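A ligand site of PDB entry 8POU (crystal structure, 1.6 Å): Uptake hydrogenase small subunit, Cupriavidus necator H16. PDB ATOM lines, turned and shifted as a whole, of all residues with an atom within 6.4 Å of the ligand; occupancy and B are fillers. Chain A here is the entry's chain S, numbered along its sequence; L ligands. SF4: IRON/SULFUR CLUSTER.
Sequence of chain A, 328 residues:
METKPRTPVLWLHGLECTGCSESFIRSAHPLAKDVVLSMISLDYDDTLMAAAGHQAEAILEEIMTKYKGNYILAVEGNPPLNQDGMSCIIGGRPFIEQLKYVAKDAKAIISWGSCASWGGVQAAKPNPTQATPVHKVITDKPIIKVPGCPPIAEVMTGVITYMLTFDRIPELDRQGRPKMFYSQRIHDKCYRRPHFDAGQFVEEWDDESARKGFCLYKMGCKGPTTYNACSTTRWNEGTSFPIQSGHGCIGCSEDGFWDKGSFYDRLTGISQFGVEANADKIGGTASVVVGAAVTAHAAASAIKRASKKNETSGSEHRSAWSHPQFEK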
ATOM      1  N   ILE A 186     -36.030  10.061 -17.537  1.00  0.00           N
ATOM      2  CA  ILE A 186     -36.017  11.415 -18.102  1.00  0.00           C
ATOM      3  C   ILE A 186     -34.794  11.618 -19.004  1.00  0.00           C
ATOM      4  O   ILE A 186     -34.891  12.155 -20.092  1.00  0.00           O
ATOM      5  CB  ILE A 186     -35.959  12.512 -17.008  1.00  0.00           C
ATOM      6  CG1 ILE A 186     -37.127  12.378 -16.008  1.00  0.00           C
ATOM      7  CG2 ILE A 186     -35.930  13.904 -17.619  1.00  0.00           C
ATOM      8  CD1 ILE A 186     -38.488  12.386 -16.628  1.00  0.00           C
ATOM      9  N   HIS A 187     -33.638  11.159 -18.505  1.00  0.00           N
ATOM     10  CA  HIS A 187     -32.339  11.284 -19.164  1.00  0.00           C
ATOM     11  C   HIS A 187     -32.236  10.598 -20.545  1.00  0.00           C
ATOM     12  O   HIS A 187     -31.418  11.004 -21.377  1.00  0.00           O
ATOM     13  CB  HIS A 187     -31.293  10.713 -18.189  1.00  0.00           C
ATOM     14  CG  HIS A 187     -29.861  10.857 -18.614  1.00  0.00           C
ATOM     15  ND1 HIS A 187     -29.145  12.005 -18.415  1.00  0.00           N
ATOM     16  CD2 HIS A 187     -28.998   9.970 -19.152  1.00  0.00           C
ATOM     17  CE1 HIS A 187     -27.911  11.837 -18.850  1.00  0.00           C
ATOM     18  NE2 HIS A 187     -27.794  10.598 -19.291  1.00  0.00           N
ATOM     19  N   ASP A 188     -33.071   9.586 -20.787  1.00  0.00           N
ATOM     20  CA  ASP A 188     -33.052   8.806 -22.043  1.00  0.00           C
ATOM     21  C   ASP A 188     -33.298   9.674 -23.282  1.00  0.00           C
ATOM     22  O   ASP A 188     -32.561   9.566 -24.265  1.00  0.00           O
ATOM     23  CB  ASP A 188     -34.107   7.688 -22.023  1.00  0.00           C
ATOM     24  CG  ASP A 188     -33.796   6.594 -20.991  1.00  0.00           C
ATOM     25  OD1 ASP A 188     -32.661   6.520 -20.493  1.00  0.00           O
ATOM     26  OD2 ASP A 188     -34.733   5.788 -20.684  1.00  0.00           O
ATOM     27  N   CYS A 190     -34.088  13.247 -22.938  1.00  0.00           N
ATOM     28  CA  CYS A 190     -33.913  14.657 -22.598  1.00  0.00           C
ATOM     29  C   CYS A 190     -33.146  15.383 -23.709  1.00  0.00           C
ATOM     30  O   CYS A 190     -32.073  14.947 -24.110  1.00  0.00           O
ATOM     31  CB  CYS A 190     -33.171  14.807 -21.263  1.00  0.00           C
ATOM     32  SG  CYS A 190     -32.800  16.530 -20.838  1.00  0.00           S
ATOM     33  N   TYR A 191     -33.710  16.489 -24.190  1.00  0.00           N
ATOM     34  CA  TYR A 191     -33.113  17.240 -25.296  1.00  0.00           C
ATOM     35  C   TYR A 191     -31.723  17.841 -24.970  1.00  0.00           C
ATOM     36  O   TYR A 191     -31.009  18.248 -25.889  1.00  0.00           O
ATOM     37  CB  TYR A 191     -34.072  18.356 -25.776  1.00  0.00           C
ATOM     38  CG  TYR A 191     -33.983  19.616 -24.935  1.00  0.00           C
ATOM     39  CD1 TYR A 191     -34.596  19.691 -23.680  1.00  0.00           C
ATOM     40  CD2 TYR A 191     -33.266  20.724 -25.386  1.00  0.00           C
ATOM     41  CE1 TYR A 191     -34.501  20.837 -22.913  1.00  0.00           C
ATOM     42  CE2 TYR A 191     -33.177  21.869 -24.610  1.00  0.00           C
ATOM     43  CZ  TYR A 191     -33.790  21.915 -23.372  1.00  0.00           C
ATOM     44  OH  TYR A 191     -33.692  23.047 -22.604  1.00  0.00           O
ATOM     45  N   ARG A 192     -31.349  17.891 -23.690  1.00  0.00           N
ATOM     46  CA  ARG A 192     -30.003  18.347 -23.279  1.00  0.00           C
ATOM     47  C   ARG A 192     -28.993  17.195 -23.263  1.00  0.00           C
ATOM     48  O   ARG A 192     -27.833  17.406 -22.958  1.00  0.00           O
ATOM     49  CB  ARG A 192     -30.044  19.015 -21.905  1.00  0.00           C
ATOM     50  CG  ARG A 192     -30.979  20.225 -21.846  1.00  0.00           C
ATOM     51  CD  ARG A 192     -30.661  21.157 -20.674  1.00  0.00           C
ATOM     52  NE  ARG A 192     -31.580  22.290 -20.626  1.00  0.00           N
ATOM     53  CZ  ARG A 192     -31.364  23.459 -20.004  1.00  0.00           C
ATOM     54  NH1 ARG A 192     -30.228  23.703 -19.351  1.00  0.00           N
ATOM     55  NH2 ARG A 192     -32.304  24.400 -20.046  1.00  0.00           N
ATOM     56  N   ARG A 193     -29.430  15.986 -23.604  1.00  0.00           N
ATOM     57  CA  ARG A 193     -28.556  14.808 -23.591  1.00  0.00           C
ATOM     58  C   ARG A 193     -27.250  14.969 -24.401  1.00  0.00           C
ATOM     59  O   ARG A 193     -26.192  14.535 -23.945  1.00  0.00           O
ATOM     60  CB  ARG A 193     -29.349  13.565 -24.031  1.00  0.00           C
ATOM     61  CG  ARG A 193     -28.596  12.249 -23.987  1.00  0.00           C
ATOM     62  CD  ARG A 193     -28.151  11.917 -22.570  1.00  0.00           C
ATOM     63  NE  ARG A 193     -27.349  10.718 -22.563  1.00  0.00           N
ATOM     64  CZ  ARG A 193     -27.820   9.474 -22.561  1.00  0.00           C
ATOM     65  NH1 ARG A 193     -29.134   9.242 -22.571  1.00  0.00           N
ATOM     66  NH2 ARG A 193     -26.971   8.457 -22.569  1.00  0.00           N
ATOM     67  N   PRO A 194     -27.323  15.576 -25.600  1.00  0.00           N
ATOM     68  CA  PRO A 194     -26.085  15.782 -26.354  1.00  0.00           C
ATOM     69  C   PRO A 194     -25.041  16.614 -25.590  1.00  0.00           C
ATOM     70  O   PRO A 194     -23.842  16.383 -25.748  1.00  0.00           O
ATOM     71  CB  PRO A 194     -26.567  16.504 -27.621  1.00  0.00           C
ATOM     72  CG  PRO A 194     -27.950  15.976 -27.808  1.00  0.00           C
ATOM     73  CD  PRO A 194     -28.519  15.874 -26.421  1.00  0.00           C
ATOM     74  N   HIS A 195     -25.496  17.553 -24.775  1.00  0.00           N
ATOM     75  CA  HIS A 195     -24.586  18.309 -23.919  1.00  0.00           C
ATOM     76  C   HIS A 195     -23.979  17.416 -22.833  1.00  0.00           C
ATOM     77  O   HIS A 195     -22.769  17.463 -22.599  1.00  0.00           O
ATOM     78  CB  HIS A 195     -25.288  19.516 -23.296  1.00  0.00           C
ATOM     79  CG  HIS A 195     -25.651  20.571 -24.296  1.00  0.00           C
ATOM     80  ND1 HIS A 195     -24.710  21.188 -25.085  1.00  0.00           N
ATOM     81  CD2 HIS A 195     -26.838  21.111 -24.632  1.00  0.00           C
ATOM     82  CE1 HIS A 195     -25.304  22.078 -25.865  1.00  0.00           C
ATOM     83  NE2 HIS A 195     -26.596  22.046 -25.610  1.00  0.00           N
ATOM     84  N   PHE A 196     -24.811  16.610 -22.176  1.00  0.00           N
ATOM     85  CA  PHE A 196     -24.316  15.631 -21.194  1.00  0.00           C
ATOM     86  C   PHE A 196     -23.239  14.741 -21.827  1.00  0.00           C
ATOM     87  O   PHE A 196     -22.160  14.584 -21.257  1.00  0.00           O
ATOM     88  CB  PHE A 196     -25.456  14.758 -20.670  1.00  0.00           C
ATOM     89  CG  PHE A 196     -25.016  13.674 -19.717  1.00  0.00           C
ATOM     90  CD1 PHE A 196     -24.594  12.442 -20.198  1.00  0.00           C
ATOM     91  CD2 PHE A 196     -25.034  13.886 -18.350  1.00  0.00           C
ATOM     92  CE1 PHE A 196     -24.197  11.436 -19.328  1.00  0.00           C
ATOM     93  CE2 PHE A 196     -24.643  12.878 -17.472  1.00  0.00           C
ATOM     94  CZ  PHE A 196     -24.223  11.661 -17.953  1.00  0.00           C
ATOM     95  N   PHE A 201     -21.740  21.237 -19.182  1.00  0.00           N
ATOM     96  CA  PHE A 201     -22.586  21.374 -18.001  1.00  0.00           C
ATOM     97  C   PHE A 201     -22.706  22.801 -17.487  1.00  0.00           C
ATOM     98  O   PHE A 201     -21.744  23.577 -17.520  1.00  0.00           O
ATOM     99  CB  PHE A 201     -22.025  20.530 -16.867  1.00  0.00           C
ATOM    100  CG  PHE A 201     -21.904  19.076 -17.185  1.00  0.00           C
ATOM    101  CD1 PHE A 201     -23.029  18.268 -17.211  1.00  0.00           C
ATOM    102  CD2 PHE A 201     -20.660  18.508 -17.456  1.00  0.00           C
ATOM    103  CE1 PHE A 201     -22.921  16.912 -17.514  1.00  0.00           C
ATOM    104  CE2 PHE A 201     -20.548  17.160 -17.754  1.00  0.00           C
ATOM    105  CZ  PHE A 201     -21.686  16.357 -17.777  1.00  0.00           C
ATOM    106  N   PHE A 214     -27.021  24.102 -21.537  1.00  0.00           N
ATOM    107  CA  PHE A 214     -26.172  22.964 -21.214  1.00  0.00           C
ATOM    108  C   PHE A 214     -26.831  22.049 -20.163  1.00  0.00           C
ATOM    109  O   PHE A 214     -27.784  22.445 -19.470  1.00  0.00           O
ATOM    110  CB  PHE A 214     -24.795  23.462 -20.725  1.00  0.00           C
ATOM    111  CG  PHE A 214     -23.817  23.826 -21.832  1.00  0.00           C
ATOM    112  CD1 PHE A 214     -24.241  24.011 -23.154  1.00  0.00           C
ATOM    113  CD2 PHE A 214     -22.476  24.014 -21.547  1.00  0.00           C
ATOM    114  CE1 PHE A 214     -23.346  24.337 -24.152  1.00  0.00           C
ATOM    115  CE2 PHE A 214     -21.577  24.348 -22.541  1.00  0.00           C
ATOM    116  CZ  PHE A 214     -22.003  24.511 -23.843  1.00  0.00           C
ATOM    117  N   CYS A 215     -26.317  20.839 -20.054  1.00  0.00           N
ATOM    118  CA  CYS A 215     -26.868  19.836 -19.160  1.00  0.00           C
ATOM    119  C   CYS A 215     -26.838  20.311 -17.698  1.00  0.00           C
ATOM    120  O   CYS A 215     -25.906  21.018 -17.279  1.00  0.00           O
ATOM    121  CB  CYS A 215     -26.119  18.526 -19.316  1.00  0.00           C
ATOM    122  SG  CYS A 215     -26.510  17.246 -18.096  1.00  0.00           S
ATOM    123  N   LEU A 216     -27.840  19.890 -16.939  1.00  0.00           N
ATOM    124  CA  LEU A 216     -28.073  20.335 -15.560  1.00  0.00           C
ATOM    125  C   LEU A 216     -27.608  19.321 -14.505  1.00  0.00           C
ATOM    126  O   LEU A 216     -27.878  19.491 -13.326  1.00  0.00           O
ATOM    127  CB  LEU A 216     -29.567  20.653 -15.366  1.00  0.00           C
ATOM    128  CG  LEU A 216     -30.031  21.877 -16.181  1.00  0.00           C
ATOM    129  CD1 LEU A 216     -31.545  21.988 -16.215  1.00  0.00           C
ATOM    130  CD2 LEU A 216     -29.432  23.140 -15.604  1.00  0.00           C
ATOM    131  N   TYR A 217     -26.915  18.271 -14.940  1.00  0.00           N
ATOM    132  CA  TYR A 217     -26.408  17.207 -14.023  1.00  0.00           C
ATOM    133  C   TYR A 217     -25.636  17.758 -12.822  1.00  0.00           C
ATOM    134  O   TYR A 217     -25.880  17.342 -11.691  1.00  0.00           O
ATOM    135  CB  TYR A 217     -25.529  16.228 -14.810  1.00  0.00           C
ATOM    136  CG  TYR A 217     -25.058  15.026 -14.024  1.00  0.00           C
ATOM    137  CD1 TYR A 217     -25.825  13.878 -13.950  1.00  0.00           C
ATOM    138  CD2 TYR A 217     -23.814  15.017 -13.402  1.00  0.00           C
ATOM    139  CE1 TYR A 217     -25.393  12.762 -13.242  1.00  0.00           C
ATOM    140  CE2 TYR A 217     -23.365  13.905 -12.694  1.00  0.00           C
ATOM    141  CZ  TYR A 217     -24.155  12.781 -12.621  1.00  0.00           C
ATOM    142  OH  TYR A 217     -23.706  11.675 -11.925  1.00  0.00           O
ATOM    143  N   LYS A 218     -24.730  18.695 -13.061  1.00  0.00           N
ATOM    144  CA  LYS A 218     -23.910  19.255 -11.973  1.00  0.00           C
ATOM    145  C   LYS A 218     -24.668  20.237 -11.074  1.00  0.00           C
ATOM    146  O   LYS A 218     -24.186  20.601 -10.008  1.00  0.00           O
ATOM    147  CB  LYS A 218     -22.629  19.888 -12.540  1.00  0.00           C
ATOM    148  CG  LYS A 218     -21.759  18.857 -13.217  1.00  0.00           C
ATOM    149  CD  LYS A 218     -20.418  19.409 -13.640  1.00  0.00           C
ATOM    150  CE  LYS A 218     -19.516  18.285 -14.120  1.00  0.00           C
ATOM    151  NZ  LYS A 218     -18.243  18.808 -14.682  1.00  0.00           N
ATOM    152  N   CYS A 221     -29.528  17.678 -11.273  1.00  0.00           N
ATOM    153  CA  CYS A 221     -30.569  17.019 -12.062  1.00  0.00           C
ATOM    154  C   CYS A 221     -30.643  15.516 -11.771  1.00  0.00           C
ATOM    155  O   CYS A 221     -29.658  14.812 -11.900  1.00  0.00           O
ATOM    156  CB  CYS A 221     -30.360  17.254 -13.553  1.00  0.00           C
ATOM    157  SG  CYS A 221     -31.722  16.568 -14.540  1.00  0.00           S
ATOM    158  N   LYS A 222     -31.822  15.038 -11.371  1.00  0.00           N
ATOM    159  CA  LYS A 222     -32.021  13.633 -11.070  1.00  0.00           C
ATOM    160  C   LYS A 222     -32.670  12.868 -12.223  1.00  0.00           C
ATOM    161  O   LYS A 222     -33.131  11.736 -12.062  1.00  0.00           O
ATOM    162  CB  LYS A 222     -32.821  13.492  -9.781  1.00  0.00           C
ATOM    163  CG  LYS A 222     -32.176  14.155  -8.570  1.00  0.00           C
ATOM    164  CD  LYS A 222     -30.721  13.731  -8.397  1.00  0.00           C
ATOM    165  CE  LYS A 222     -30.138  14.153  -7.065  1.00  0.00           C
ATOM    166  NZ  LYS A 222     -30.208  15.617  -6.770  1.00  0.00           N
ATOM    167  N   GLY A 223     -32.653  13.463 -13.420  1.00  0.00           N
ATOM    168  CA  GLY A 223     -33.152  12.806 -14.624  1.00  0.00           C
ATOM    169  C   GLY A 223     -32.589  11.408 -14.902  1.00  0.00           C
ATOM    170  O   GLY A 223     -33.325  10.537 -15.375  1.00  0.00           O
ATOM    171  N   PRO A 224     -31.277  11.195 -14.629  1.00  0.00           N
ATOM    172  CA  PRO A 224     -30.676   9.869 -14.845  1.00  0.00           C
ATOM    173  C   PRO A 224     -31.234   8.722 -14.000  1.00  0.00           C
ATOM    174  O   PRO A 224     -31.028   7.564 -14.354  1.00  0.00           O
ATOM    175  CB  PRO A 224     -29.196  10.099 -14.542  1.00  0.00           C
ATOM    176  CG  PRO A 224     -28.980  11.536 -14.900  1.00  0.00           C
ATOM    177  CD  PRO A 224     -30.238  12.224 -14.462  1.00  0.00           C
ATOM    178  N   PHE A 241     -40.892  21.463 -19.784  1.00  0.00           N
ATOM    179  CA  PHE A 241     -40.732  20.592 -18.620  1.00  0.00           C
ATOM    180  C   PHE A 241     -39.611  21.194 -17.756  1.00  0.00           C
ATOM    181  O   PHE A 241     -38.941  22.150 -18.175  1.00  0.00           O
ATOM    182  CB  PHE A 241     -40.569  19.116 -19.035  1.00  0.00           C
ATOM    183  CG  PHE A 241     -39.242  18.750 -19.616  1.00  0.00           C
ATOM    184  CD1 PHE A 241     -38.822  19.243 -20.859  1.00  0.00           C
ATOM    185  CD2 PHE A 241     -38.414  17.818 -18.971  1.00  0.00           C
ATOM    186  CE1 PHE A 241     -37.603  18.863 -21.421  1.00  0.00           C
ATOM    187  CE2 PHE A 241     -37.212  17.428 -19.521  1.00  0.00           C
ATOM    188  CZ  PHE A 241     -36.803  17.947 -20.756  1.00  0.00           C
ATOM    189  N   ILE A 243     -36.572  20.705 -16.934  1.00  0.00           N
ATOM    190  CA  ILE A 243     -35.249  20.878 -17.520  1.00  0.00           C
ATOM    191  C   ILE A 243     -35.259  21.914 -18.653  1.00  0.00           C
ATOM    192  O   ILE A 243     -34.346  22.738 -18.728  1.00  0.00           O
ATOM    193  CB  ILE A 243     -34.697  19.520 -17.961  1.00  0.00           C
ATOM    194  CG1 ILE A 243     -34.357  18.685 -16.713  1.00  0.00           C
ATOM    195  CG2 ILE A 243     -33.492  19.669 -18.884  1.00  0.00           C
ATOM    196  CD1 ILE A 243     -34.482  17.190 -16.917  1.00  0.00           C
ATOM    197  N   GLY A 248     -33.018  21.490 -12.868  1.00  0.00           N
ATOM    198  CA  GLY A 248     -32.887  20.053 -12.941  1.00  0.00           C
ATOM    199  C   GLY A 248     -34.137  19.353 -12.423  1.00  0.00           C
ATOM    200  O   GLY A 248     -34.856  19.867 -11.570  1.00  0.00           O
ATOM    201  N   CYS A 249     -34.382  18.173 -12.944  1.00  0.00           N
ATOM    202  CA  CYS A 249     -35.355  17.282 -12.339  1.00  0.00           C
ATOM    203  C   CYS A 249     -34.939  17.067 -10.877  1.00  0.00           C
ATOM    204  O   CYS A 249     -33.743  16.875 -10.574  1.00  0.00           O
ATOM    205  CB  CYS A 249     -35.377  15.971 -13.125  1.00  0.00           C
ATOM    206  SG  CYS A 249     -36.304  14.586 -12.428  1.00  0.00           S
HETATM  207 FE1  SF4 L   1     -29.786  13.999 -18.225  1.00  0.00          FE
HETATM  208 FE2  SF4 L   1     -30.730  16.058 -16.571  1.00  0.00          FE
HETATM  209 FE3  SF4 L   1     -31.164  16.141 -19.253  1.00  0.00          FE
HETATM  210 FE4  SF4 L   1     -28.633  16.469 -18.266  1.00  0.00          FE
HETATM  211  S1  SF4 L   1     -30.418  17.861 -18.002  1.00  0.00           S
HETATM  212  S2  SF4 L   1     -29.265  15.214 -20.080  1.00  0.00           S
HETATM  213  S3  SF4 L   1     -28.706  15.073 -16.473  1.00  0.00           S
HETATM  214  S4  SF4 L   1     -31.960  14.555 -17.746  1.00  0.00           S
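Arg 192 touches the ligand (C to S2, 3.8 Å). Phe 196 touches the ligand (CB to S2, 3.9 Å). Tyr 217 touches the ligand. CA of Gly 223 touches S4 of the ligand, at 3.8 Å. CD of Pro 224 touches S3 of the ligand, 3.8 Å away. Ile 243 touches the ligand. Hydrophobic or aromatic side chains within 4 Å of the ligand: His 187, Phe 196, Leu 216, Tyr 217, Pro 224 and Ile 243. The nearest printed residue that does not touch the ligand is Ile 186 (4.03 Å).
The side-chain sulfur (SG) of Cys 215 sits close to the backbone NH (N) of Tyr 217 (3.3 Å). The side-chain sulfur (SG) of Cys 190 lies close to the backbone NH (N) of Arg 192 (3.5 Å). N of Cys 221 lies within hydrogen-bond range of O of Leu 216. The side-chain sulfur of Cys 221 sits close to the backbone NH of Gly 223 (3.4 Å). The backbone NH (N) of Cys 249 sits close to the side-chain sulfur (SG) of Cys 221 (3.5 Å). NH2 of Arg 192 is in hydrogen-bond range of O of Ile 243, 2.9 Å away. The side-chain hydroxyl (OH) of Tyr 191 is in hydrogen-bond range of the guanidinium group (NE) of Arg 192 (3.0 Å). The backbone carbonyl oxygen (O) of Gly 223 lies within hydrogen-bond range of the backbone NH (N) of Ile 186.
A ring nitrogen (ND1) of His 187 binds an iron atom (FE1) of the ligand, at 2.1 Å. An iron atom (FE4) of the ligand is bound by the side-chain sulfur (SG) of Cys 215 (2.3 Å). FE3 of the ligand is bound by SG of Cys 190 (2.3 Å). The side-chain sulfur of Cys 221 is bound to an iron atom (FE2) of the ligand. N of Leu 216 lies close to S1 of the ligand (3.4 Å). The backbone NH of Arg 193 lies close to a sulfur (S2) of the ligand, 3.6 Å away.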
